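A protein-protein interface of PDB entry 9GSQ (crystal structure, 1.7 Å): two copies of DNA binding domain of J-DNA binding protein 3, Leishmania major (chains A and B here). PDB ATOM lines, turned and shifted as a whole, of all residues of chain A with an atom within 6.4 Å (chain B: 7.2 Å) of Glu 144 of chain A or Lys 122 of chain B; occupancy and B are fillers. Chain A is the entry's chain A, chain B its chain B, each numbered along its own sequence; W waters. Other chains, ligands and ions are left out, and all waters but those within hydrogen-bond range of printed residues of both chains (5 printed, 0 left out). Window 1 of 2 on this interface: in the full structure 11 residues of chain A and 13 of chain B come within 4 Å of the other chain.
N of Glu 144 of chain A is in hydrogen-bond range of OD1 of Asp 114 of chain B (3.1 Å). NZ of Lys 122 of chain B lies within salt-bridge range of OE1 of Glu 144 of chain A (2.6 Å). The side-chain hydroxyl of Thr 145 of chain A lies within hydrogen-bond range of the side-chain carboxylate of Asp 114 of chain B, 2.6 Å away.
NZ of Lys 122 of chain B is in hydrogen-bond range of O of Tyr 113 of chain B. OH of Tyr 113 of chain B is in hydrogen-bond range of O of Pro 123 of chain B (2.6 Å). The backbone NH (N) of Trp 125 of chain B is in hydrogen-bond range of the side-chain hydroxyl (OH) of Tyr 113 of chain B. The backbone carbonyl oxygen (O) of Leu 116 of chain B is in hydrogen-bond range of the side-chain amino group (NZ) of Lys 122 of chain B, at 2.9 Å.
Ile 137 of chain A touches Tyr 21 of chain B (O to OH, 3.5 Å). CG2 of Ile 137 of chain A touches CG of Pro 118 of chain B (3.5 Å). Asp 114 of chain B touches Pro 143 of chain A. Tyr 113 of chain B touches Glu 144 of chain A. Glu 144 of chain A touches Leu 116 of chain B (OE1 to O, 3.9 Å). Glu 144 of chain A touches Pro 118 of chain B (OE1 to CG, 3.6 Å). Thr 145 of chain A touches Tyr 113 of chain B. Ser 149 of chain A touches Leu 124 of chain B.
Glu 144 of chain A touches just these residues of chain B: Tyr 113 (3.9 Å), Asp 114 (3.1 Å), Leu 116 (3.9 Å), Pro 118 (3.6 Å) and Lys 122 (2.6 Å). Printed residues of chain A within 4 Å of Leu 116 of chain B: Glu 144 (3.9 Å). Printed residues of chain A within 4 Å of Pro 118 of chain B: Ile 137 (3.5 Å) and Glu 144 (3.6 Å). Of chain A, only Glu 144 (2.6 Å) comes within 4 Å of Lys 122 of chain B. Pro 123 of chain B touches none of the printed residues of chain A. Of the printed residues of chain A, Leu 124 of chain B touches Ser 149 (3.3 Å). The nearest residue of chain A that does not touch Lys 122 of chain B is Ser 149 of chain A (5.2 Å).
Along chain A the printed residues that touch a printed residue of chain B span positions 137 to 149. Hydrophobic or aromatic side chains of chain B that line the printed part of chain A: Tyr 21, Tyr 113, Pro 118 and Leu 124. Among the printed residues, 11 pairs touch across the chains. Among the printed residues, Asp or Glu carboxylates within 4 Å of a Lys or Arg side-chain nitrogen of the other chain: Glu 144 of chain A with Lys 122 of chain B (2.6 Å).
No position is printed for both chains. Of the 11 pairs that touch across the chains among the printed residues, none has its exchanged pair printed and touching as well.
Water W4 lies within hydrogen-bond range of the side-chain hydroxyl of Tyr 21 of chain B (2.5 Å) and the backbone carbonyl oxygen of Val 142 of chain A (2.9 Å). Water W5 lies within hydrogen-bond range of O of Lys 122 of chain B (2.6 Å) and OG of Ser 149 of chain A (2.8 Å). Water W3 bridges the backbone carbonyl oxygen of Asp 114 of chain B and the side-chain carboxylate of Glu 144 of chain A. Water W1 bridges OE2 of Glu 144 of chain A (2.7 Å) and N of Gly 119 of chain B (3.2 Å). Water W2 lies within hydrogen-bond range of OG of Ser 149 of chain A, OE2 of Glu 144 of chain A and OH of Tyr 113 of chain B.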
ATOM      1  N   ILE A 137     -18.905  13.537  39.196  1.00  0.00           N
ATOM      2  CA  ILE A 137     -19.506  14.369  38.166  1.00  0.00           C
ATOM      3  C   ILE A 137     -20.996  14.573  38.432  1.00  0.00           C
ATOM      4  O   ILE A 137     -21.461  15.701  38.400  1.00  0.00           O
ATOM      5  CB  ILE A 137     -19.224  13.751  36.775  1.00  0.00           C
ATOM      6  CG1 ILE A 137     -17.747  13.782  36.477  1.00  0.00           C
ATOM      7  CG2 ILE A 137     -20.037  14.446  35.687  1.00  0.00           C
ATOM      8  CD1 ILE A 137     -17.285  12.897  35.326  1.00  0.00           C
ATOM      9  N   VAL A 142     -21.090  19.564  37.497  1.00  0.00           N
ATOM     10  CA  VAL A 142     -20.185  20.370  36.693  1.00  0.00           C
ATOM     11  C   VAL A 142     -20.149  19.728  35.307  1.00  0.00           C
ATOM     12  O   VAL A 142     -19.907  18.528  35.198  1.00  0.00           O
ATOM     13  CB  VAL A 142     -18.789  20.481  37.314  1.00  0.00           C
ATOM     14  CG1 VAL A 142     -17.794  21.164  36.374  1.00  0.00           C
ATOM     15  CG2 VAL A 142     -18.895  21.199  38.646  1.00  0.00           C
ATOM     16  N   PRO A 143     -20.371  20.492  34.214  1.00  0.00           N
ATOM     17  CA  PRO A 143     -20.395  19.902  32.875  1.00  0.00           C
ATOM     18  C   PRO A 143     -19.065  19.247  32.515  1.00  0.00           C
ATOM     19  O   PRO A 143     -17.998  19.825  32.715  1.00  0.00           O
ATOM     20  CB  PRO A 143     -20.658  21.102  31.936  1.00  0.00           C
ATOM     21  CG  PRO A 143     -21.137  22.209  32.814  1.00  0.00           C
ATOM     22  CD  PRO A 143     -20.618  21.943  34.197  1.00  0.00           C
ATOM     23  N   GLU A 144     -19.150  18.067  31.911  1.00  0.00           N
ATOM     24  CA  GLU A 144     -17.963  17.343  31.495  1.00  0.00           C
ATOM     25  C   GLU A 144     -17.188  18.018  30.373  1.00  0.00           C
ATOM     26  O   GLU A 144     -15.995  17.780  30.248  1.00  0.00           O
ATOM     27  CB  GLU A 144     -18.312  15.924  31.090  1.00  0.00           C
ATOM     28  CG  GLU A 144     -18.504  15.022  32.276  1.00  0.00           C
ATOM     29  CD  GLU A 144     -19.210  13.731  31.906  1.00  0.00           C
ATOM     30  OE1 GLU A 144     -20.464  13.749  31.871  1.00  0.00           O
ATOM     31  OE2 GLU A 144     -18.511  12.738  31.604  1.00  0.00           O
ATOM     32  N   THR A 145     -17.843  18.883  29.588  1.00  0.00           N
ATOM     33  CA  THR A 145     -17.089  19.694  28.639  1.00  0.00           C
ATOM     34  C   THR A 145     -16.149  20.672  29.338  1.00  0.00           C
ATOM     35  O   THR A 145     -15.180  21.122  28.731  1.00  0.00           O
ATOM     36  CB  THR A 145     -17.982  20.433  27.656  1.00  0.00           C
ATOM     37  OG1 THR A 145     -18.899  21.235  28.368  1.00  0.00           O
ATOM     38  CG2 THR A 145     -18.725  19.475  26.743  1.00  0.00           C
ATOM     39  N   MET A 146     -16.447  20.994  30.599  1.00  0.00           N
ATOM     40  CA  MET A 146     -15.609  21.887  31.387  1.00  0.00           C
ATOM     41  C   MET A 146     -14.606  21.104  32.225  1.00  0.00           C
ATOM     42  O   MET A 146     -13.437  21.467  32.312  1.00  0.00           O
ATOM     43  CB  MET A 146     -16.470  22.755  32.319  1.00  0.00           C
ATOM     44  CG  MET A 146     -17.362  23.722  31.638  1.00  0.00           C
ATOM     45  SD  MET A 146     -16.425  25.027  30.882  1.00  0.00           S
ATOM     46  CE  MET A 146     -16.492  24.497  29.166  1.00  0.00           C
ATOM     47  N   LEU A 147     -15.074  20.022  32.848  1.00  0.00           N
ATOM     48  CA  LEU A 147     -14.228  19.171  33.656  1.00  0.00           C
ATOM     49  C   LEU A 147     -14.522  17.728  33.279  1.00  0.00           C
ATOM     50  O   LEU A 147     -15.542  17.164  33.688  1.00  0.00           O
ATOM     51  CB  LEU A 147     -14.469  19.445  35.143  1.00  0.00           C
ATOM     52  CG  LEU A 147     -13.794  18.488  36.134  1.00  0.00           C
ATOM     53  CD1 LEU A 147     -12.327  18.415  35.884  1.00  0.00           C
ATOM     54  CD2 LEU A 147     -14.019  18.944  37.553  1.00  0.00           C
ATOM     55  N   SER A 148     -13.599  17.152  32.503  1.00  0.00           N
ATOM     56  CA  SER A 148     -13.824  15.866  31.879  1.00  0.00           C
ATOM     57  C   SER A 148     -13.455  14.700  32.784  1.00  0.00           C
ATOM     58  O   SER A 148     -12.624  14.834  33.687  1.00  0.00           O
ATOM     59  CB  SER A 148     -12.996  15.734  30.607  1.00  0.00           C
ATOM     60  OG  SER A 148     -11.616  15.750  30.923  1.00  0.00           O
ATOM     61  N   SER A 149     -13.985  13.531  32.422  1.00  0.00           N
ATOM     62  CA  SER A 149     -13.593  12.288  33.059  1.00  0.00           C
ATOM     63  C   SER A 149     -12.099  12.057  32.891  1.00  0.00           C
ATOM     64  O   SER A 149     -11.457  11.456  33.755  1.00  0.00           O
ATOM     65  CB  SER A 149     -14.391  11.110  32.507  1.00  0.00           C
ATOM     66  OG  SER A 149     -14.202  11.024  31.103  1.00  0.00           O
ATOM     67  N   TYR B  21     -30.019  13.791  34.101  1.00  0.00           N
ATOM     68  CA  TYR B  21     -29.152  13.215  33.084  1.00  0.00           C
ATOM     69  C   TYR B  21     -29.922  12.256  32.175  1.00  0.00           C
ATOM     70  O   TYR B  21     -30.855  11.567  32.599  1.00  0.00           O
ATOM     71  CB  TYR B  21     -27.974  12.487  33.756  1.00  0.00           C
ATOM     72  CG  TYR B  21     -26.946  13.406  34.378  1.00  0.00           C
ATOM     73  CD1 TYR B  21     -25.957  13.989  33.610  1.00  0.00           C
ATOM     74  CD2 TYR B  21     -26.945  13.667  35.744  1.00  0.00           C
ATOM     75  CE1 TYR B  21     -24.999  14.815  34.170  1.00  0.00           C
ATOM     76  CE2 TYR B  21     -26.023  14.525  36.309  1.00  0.00           C
ATOM     77  CZ  TYR B  21     -25.032  15.083  35.530  1.00  0.00           C
ATOM     78  OH  TYR B  21     -24.100  15.921  36.082  1.00  0.00           O
ATOM     79  N   LEU B  24     -27.461   6.569  29.049  1.00  0.00           N
ATOM     80  CA  LEU B  24     -26.727   6.206  27.852  1.00  0.00           C
ATOM     81  C   LEU B  24     -27.362   4.995  27.178  1.00  0.00           C
ATOM     82  O   LEU B  24     -28.008   4.173  27.828  1.00  0.00           O
ATOM     83  CB  LEU B  24     -25.285   5.923  28.237  1.00  0.00           C
ATOM     84  CG  LEU B  24     -24.470   7.157  28.602  1.00  0.00           C
ATOM     85  CD1 LEU B  24     -23.231   6.789  29.382  1.00  0.00           C
ATOM     86  CD2 LEU B  24     -24.072   7.897  27.382  1.00  0.00           C
ATOM     87  N   LEU B  27     -23.554   0.286  26.376  1.00  0.00           N
ATOM     88  CA  LEU B  27     -22.138   0.582  26.266  1.00  0.00           C
ATOM     89  C   LEU B  27     -21.344  -0.566  26.874  1.00  0.00           C
ATOM     90  O   LEU B  27     -21.125  -0.605  28.083  1.00  0.00           O
ATOM     91  CB  LEU B  27     -21.795   1.890  26.986  1.00  0.00           C
ATOM     92  CG  LEU B  27     -22.223   3.151  26.255  1.00  0.00           C
ATOM     93  CD1 LEU B  27     -21.838   4.373  27.039  1.00  0.00           C
ATOM     94  CD2 LEU B  27     -21.621   3.196  24.841  1.00  0.00           C
ATOM     95  N   MET B  33     -19.675   2.233  21.470  1.00  0.00           N
ATOM     96  CA  MET B  33     -19.188   3.551  21.839  1.00  0.00           C
ATOM     97  C   MET B  33     -19.304   4.520  20.663  1.00  0.00           C
ATOM     98  O   MET B  33     -19.685   5.674  20.845  1.00  0.00           O
ATOM     99  CB  MET B  33     -17.740   3.470  22.336  1.00  0.00           C
ATOM    100  CG  MET B  33     -17.257   4.765  22.943  1.00  0.00           C
ATOM    101  SD  MET B  33     -16.201   4.491  24.384  1.00  0.00           S
ATOM    102  CE  MET B  33     -16.858   2.989  24.943  1.00  0.00           C
ATOM    103  N   VAL B  36     -23.120   6.028  19.914  1.00  0.00           N
ATOM    104  CA  VAL B  36     -23.898   6.674  20.957  1.00  0.00           C
ATOM    105  C   VAL B  36     -24.672   7.861  20.399  1.00  0.00           C
ATOM    106  O   VAL B  36     -25.869   7.981  20.621  1.00  0.00           O
ATOM    107  CB  VAL B  36     -22.993   7.111  22.150  1.00  0.00           C
ATOM    108  CG1 VAL B  36     -23.764   8.007  23.111  1.00  0.00           C
ATOM    109  CG2 VAL B  36     -22.414   5.911  22.872  1.00  0.00           C
ATOM    110  N   LEU B 112     -25.973  18.374  24.728  1.00  0.00           N
ATOM    111  CA  LEU B 112     -26.362  16.980  24.804  1.00  0.00           C
ATOM    112  C   LEU B 112     -25.301  16.158  25.523  1.00  0.00           C
ATOM    113  O   LEU B 112     -25.629  15.382  26.418  1.00  0.00           O
ATOM    114  CB  LEU B 112     -26.637  16.443  23.415  1.00  0.00           C
ATOM    115  CG  LEU B 112     -26.969  14.970  23.327  1.00  0.00           C
ATOM    116  CD1 LEU B 112     -28.267  14.646  24.160  1.00  0.00           C
ATOM    117  CD2 LEU B 112     -27.130  14.572  21.845  1.00  0.00           C
ATOM    118  N   TYR B 113     -24.038  16.341  25.134  1.00  0.00           N
ATOM    119  CA  TYR B 113     -22.945  15.611  25.742  1.00  0.00           C
ATOM    120  C   TYR B 113     -22.951  15.801  27.259  1.00  0.00           C
ATOM    121  O   TYR B 113     -22.870  14.826  28.018  1.00  0.00           O
ATOM    122  CB  TYR B 113     -21.624  16.066  25.182  1.00  0.00           C
ATOM    123  CG  TYR B 113     -20.472  15.284  25.757  1.00  0.00           C
ATOM    124  CD1 TYR B 113     -20.230  13.991  25.359  1.00  0.00           C
ATOM    125  CD2 TYR B 113     -19.666  15.822  26.746  1.00  0.00           C
ATOM    126  CE1 TYR B 113     -19.199  13.241  25.909  1.00  0.00           C
ATOM    127  CE2 TYR B 113     -18.660  15.071  27.349  1.00  0.00           C
ATOM    128  CZ  TYR B 113     -18.418  13.779  26.915  1.00  0.00           C
ATOM    129  OH  TYR B 113     -17.389  13.026  27.445  1.00  0.00           O
ATOM    130  N   ASP B 114     -23.109  17.054  27.691  1.00  0.00           N
ATOM    131  CA  ASP B 114     -23.046  17.369  29.107  1.00  0.00           C
ATOM    132  C   ASP B 114     -24.233  16.792  29.880  1.00  0.00           C
ATOM    133  O   ASP B 114     -24.102  16.516  31.065  1.00  0.00           O
ATOM    134  CB  ASP B 114     -22.926  18.871  29.293  1.00  0.00           C
ATOM    135  CG  ASP B 114     -21.522  19.347  29.027  1.00  0.00           C
ATOM    136  OD1 ASP B 114     -20.578  18.538  29.229  1.00  0.00           O
ATOM    137  OD2 ASP B 114     -21.354  20.519  28.570  1.00  0.00           O
ATOM    138  N   SER B 115     -25.360  16.564  29.193  1.00  0.00           N
ATOM    139  CA  SER B 115     -26.558  15.986  29.795  1.00  0.00           C
ATOM    140  C   SER B 115     -26.558  14.460  29.854  1.00  0.00           C
ATOM    141  O   SER B 115     -27.458  13.858  30.444  1.00  0.00           O
ATOM    142  CB  SER B 115     -27.815  16.449  29.051  1.00  0.00           C
ATOM    143  OG  SER B 115     -27.929  15.889  27.747  1.00  0.00           O
ATOM    144  N   LEU B 116     -25.583  13.812  29.208  1.00  0.00           N
ATOM    145  CA  LEU B 116     -25.560  12.362  29.185  1.00  0.00           C
ATOM    146  C   LEU B 116     -25.000  11.820  30.494  1.00  0.00           C
ATOM    147  O   LEU B 116     -23.964  12.278  30.977  1.00  0.00           O
ATOM    148  CB  LEU B 116     -24.714  11.818  28.042  1.00  0.00           C
ATOM    149  CG  LEU B 116     -25.156  12.197  26.661  1.00  0.00           C
ATOM    150  CD1 LEU B 116     -24.193  11.632  25.640  1.00  0.00           C
ATOM    151  CD2 LEU B 116     -26.505  11.719  26.419  1.00  0.00           C
ATOM    152  N   GLN B 117     -25.693  10.817  31.029  1.00  0.00           N
ATOM    153  CA  GLN B 117     -25.292  10.137  32.247  1.00  0.00           C
ATOM    154  C   GLN B 117     -23.808   9.791  32.198  1.00  0.00           C
ATOM    155  O   GLN B 117     -23.360   9.036  31.333  1.00  0.00           O
ATOM    156  CB  GLN B 117     -26.142   8.870  32.387  1.00  0.00           C
ATOM    157  CG  GLN B 117     -25.855   8.048  33.603  1.00  0.00           C
ATOM    158  CD  GLN B 117     -26.306   8.738  34.865  1.00  0.00           C
ATOM    159  OE1 GLN B 117     -27.420   9.276  34.971  1.00  0.00           O
ATOM    160  NE2 GLN B 117     -25.444   8.735  35.858  1.00  0.00           N
ATOM    161  N   PRO B 118     -22.982  10.336  33.118  1.00  0.00           N
ATOM    162  CA  PRO B 118     -21.588   9.927  33.224  1.00  0.00           C
ATOM    163  C   PRO B 118     -21.404   8.437  33.498  1.00  0.00           C
ATOM    164  O   PRO B 118     -22.213   7.825  34.184  1.00  0.00           O
ATOM    165  CB  PRO B 118     -21.092  10.756  34.432  1.00  0.00           C
ATOM    166  CG  PRO B 118     -22.082  11.918  34.499  1.00  0.00           C
ATOM    167  CD  PRO B 118     -23.351  11.382  34.082  1.00  0.00           C
ATOM    168  N   GLY B 119     -20.313   7.889  32.974  1.00  0.00           N
ATOM    169  CA  GLY B 119     -19.912   6.534  33.308  1.00  0.00           C
ATOM    170  C   GLY B 119     -18.555   6.207  32.717  1.00  0.00           C
ATOM    171  O   GLY B 119     -18.079   6.903  31.820  1.00  0.00           O
ATOM    172  N   PRO B 120     -17.932   5.082  33.146  1.00  0.00           N
ATOM    173  CA  PRO B 120     -16.609   4.689  32.664  1.00  0.00           C
ATOM    174  C   PRO B 120     -16.485   4.541  31.152  1.00  0.00           C
ATOM    175  O   PRO B 120     -15.414   4.765  30.588  1.00  0.00           O
ATOM    176  CB  PRO B 120     -16.384   3.325  33.347  1.00  0.00           C
ATOM    177  CG  PRO B 120     -17.331   3.297  34.479  1.00  0.00           C
ATOM    178  CD  PRO B 120     -18.508   4.111  34.088  1.00  0.00           C
ATOM    179  N   LEU B 121     -17.600   4.197  30.494  1.00  0.00           N
ATOM    180  CA  LEU B 121     -17.576   3.986  29.057  1.00  0.00           C
ATOM    181  C   LEU B 121     -18.207   5.122  28.260  1.00  0.00           C
ATOM    182  O   LEU B 121     -18.298   5.038  27.040  1.00  0.00           O
ATOM    183  CB  LEU B 121     -18.239   2.619  28.691  1.00  0.00           C
ATOM    184  CG  LEU B 121     -17.398   1.375  29.003  1.00  0.00           C
ATOM    185  CD1 LEU B 121     -17.825   0.203  28.154  1.00  0.00           C
ATOM    186  CD2 LEU B 121     -15.941   1.603  28.796  1.00  0.00           C
ATOM    187  N   LYS B 122     -18.640   6.196  28.934  1.00  0.00           N
ATOM    188  CA  LYS B 122     -19.134   7.358  28.207  1.00  0.00           C
ATOM    189  C   LYS B 122     -17.984   7.860  27.343  1.00  0.00           C
ATOM    190  O   LYS B 122     -16.873   8.067  27.840  1.00  0.00           O
ATOM    191  CB  LYS B 122     -19.639   8.447  29.157  1.00  0.00           C
ATOM    192  CG  LYS B 122     -20.099   9.708  28.443  1.00  0.00           C
ATOM    193  CD  LYS B 122     -20.692  10.705  29.375  1.00  0.00           C
ATOM    194  CE  LYS B 122     -20.898  12.024  28.711  1.00  0.00           C
ATOM    195  NZ  LYS B 122     -21.526  12.999  29.629  1.00  0.00           N
ATOM    196  N   PRO B 123     -18.180   8.053  26.021  1.00  0.00           N
ATOM    197  CA  PRO B 123     -17.108   8.560  25.178  1.00  0.00           C
ATOM    198  C   PRO B 123     -16.610   9.911  25.673  1.00  0.00           C
ATOM    199  O   PRO B 123     -17.376  10.701  26.239  1.00  0.00           O
ATOM    200  CB  PRO B 123     -17.740   8.660  23.783  1.00  0.00           C
ATOM    201  CG  PRO B 123     -19.139   8.425  23.963  1.00  0.00           C
ATOM    202  CD  PRO B 123     -19.416   7.793  25.272  1.00  0.00           C
ATOM    203  N   LEU B 124     -15.320  10.162  25.433  1.00  0.00           N
ATOM    204  CA  LEU B 124     -14.756  11.470  25.688  1.00  0.00           C
ATOM    205  C   LEU B 124     -15.337  12.446  24.672  1.00  0.00           C
ATOM    206  O   LEU B 124     -15.808  12.041  23.604  1.00  0.00           O
ATOM    207  CB  LEU B 124     -13.248  11.417  25.592  1.00  0.00           C
ATOM    208  CG  LEU B 124     -12.581  10.573  26.649  1.00  0.00           C
ATOM    209  CD1 LEU B 124     -11.083  10.691  26.525  1.00  0.00           C
ATOM    210  CD2 LEU B 124     -13.064  10.960  28.049  1.00  0.00           C
ATOM    211  N   TRP B 125     -15.354  13.725  25.038  1.00  0.00           N
ATOM    212  CA  TRP B 125     -15.918  14.752  24.166  1.00  0.00           C
ATOM    213  C   TRP B 125     -15.402  14.708  22.722  1.00  0.00           C
ATOM    214  O   TRP B 125     -16.194  14.735  21.771  1.00  0.00           O
ATOM    215  CB  TRP B 125     -15.627  16.134  24.771  1.00  0.00           C
ATOM    216  CG  TRP B 125     -15.890  17.270  23.840  1.00  0.00           C
ATOM    217  CD1 TRP B 125     -14.969  18.112  23.298  1.00  0.00           C
ATOM    218  CD2 TRP B 125     -17.164  17.648  23.281  1.00  0.00           C
ATOM    219  NE1 TRP B 125     -15.584  19.000  22.442  1.00  0.00           N
ATOM    220  CE2 TRP B 125     -16.937  18.756  22.440  1.00  0.00           C
ATOM    221  CE3 TRP B 125     -18.474  17.181  23.443  1.00  0.00           C
ATOM    222  CZ2 TRP B 125     -17.959  19.385  21.737  1.00  0.00           C
ATOM    223  CZ3 TRP B 125     -19.487  17.797  22.741  1.00  0.00           C
ATOM    224  CH2 TRP B 125     -19.234  18.900  21.917  1.00  0.00           C
ATOM    225  N   PHE B 128     -16.956  11.901  20.932  1.00  0.00           N
ATOM    226  CA  PHE B 128     -18.376  12.113  20.746  1.00  0.00           C
ATOM    227  C   PHE B 128     -18.652  13.116  19.631  1.00  0.00           C
ATOM    228  O   PHE B 128     -19.455  12.840  18.746  1.00  0.00           O
ATOM    229  CB  PHE B 128     -18.990  12.594  22.060  1.00  0.00           C
ATOM    230  CG  PHE B 128     -20.494  12.715  22.078  1.00  0.00           C
ATOM    231  CD1 PHE B 128     -21.287  11.606  22.249  1.00  0.00           C
ATOM    232  CD2 PHE B 128     -21.113  13.964  22.012  1.00  0.00           C
ATOM    233  CE1 PHE B 128     -22.665  11.723  22.305  1.00  0.00           C
ATOM    234  CE2 PHE B 128     -22.491  14.068  22.092  1.00  0.00           C
ATOM    235  CZ  PHE B 128     -23.254  12.947  22.209  1.00  0.00           C
HETATM  236  O   HOH W   1     -18.230  10.121  32.138  1.00  0.00           O
HETATM  237  O   HOH W   2     -15.866  13.180  30.210  1.00  0.00           O
HETATM  238  O   HOH W   3     -21.729  16.258  32.173  1.00  0.00           O
HETATM  239  O   HOH W   4     -22.332  17.025  34.737  1.00  0.00           O
HETATM  240  O   HOH W   5     -16.189   9.581  29.805  1.00  0.00           O
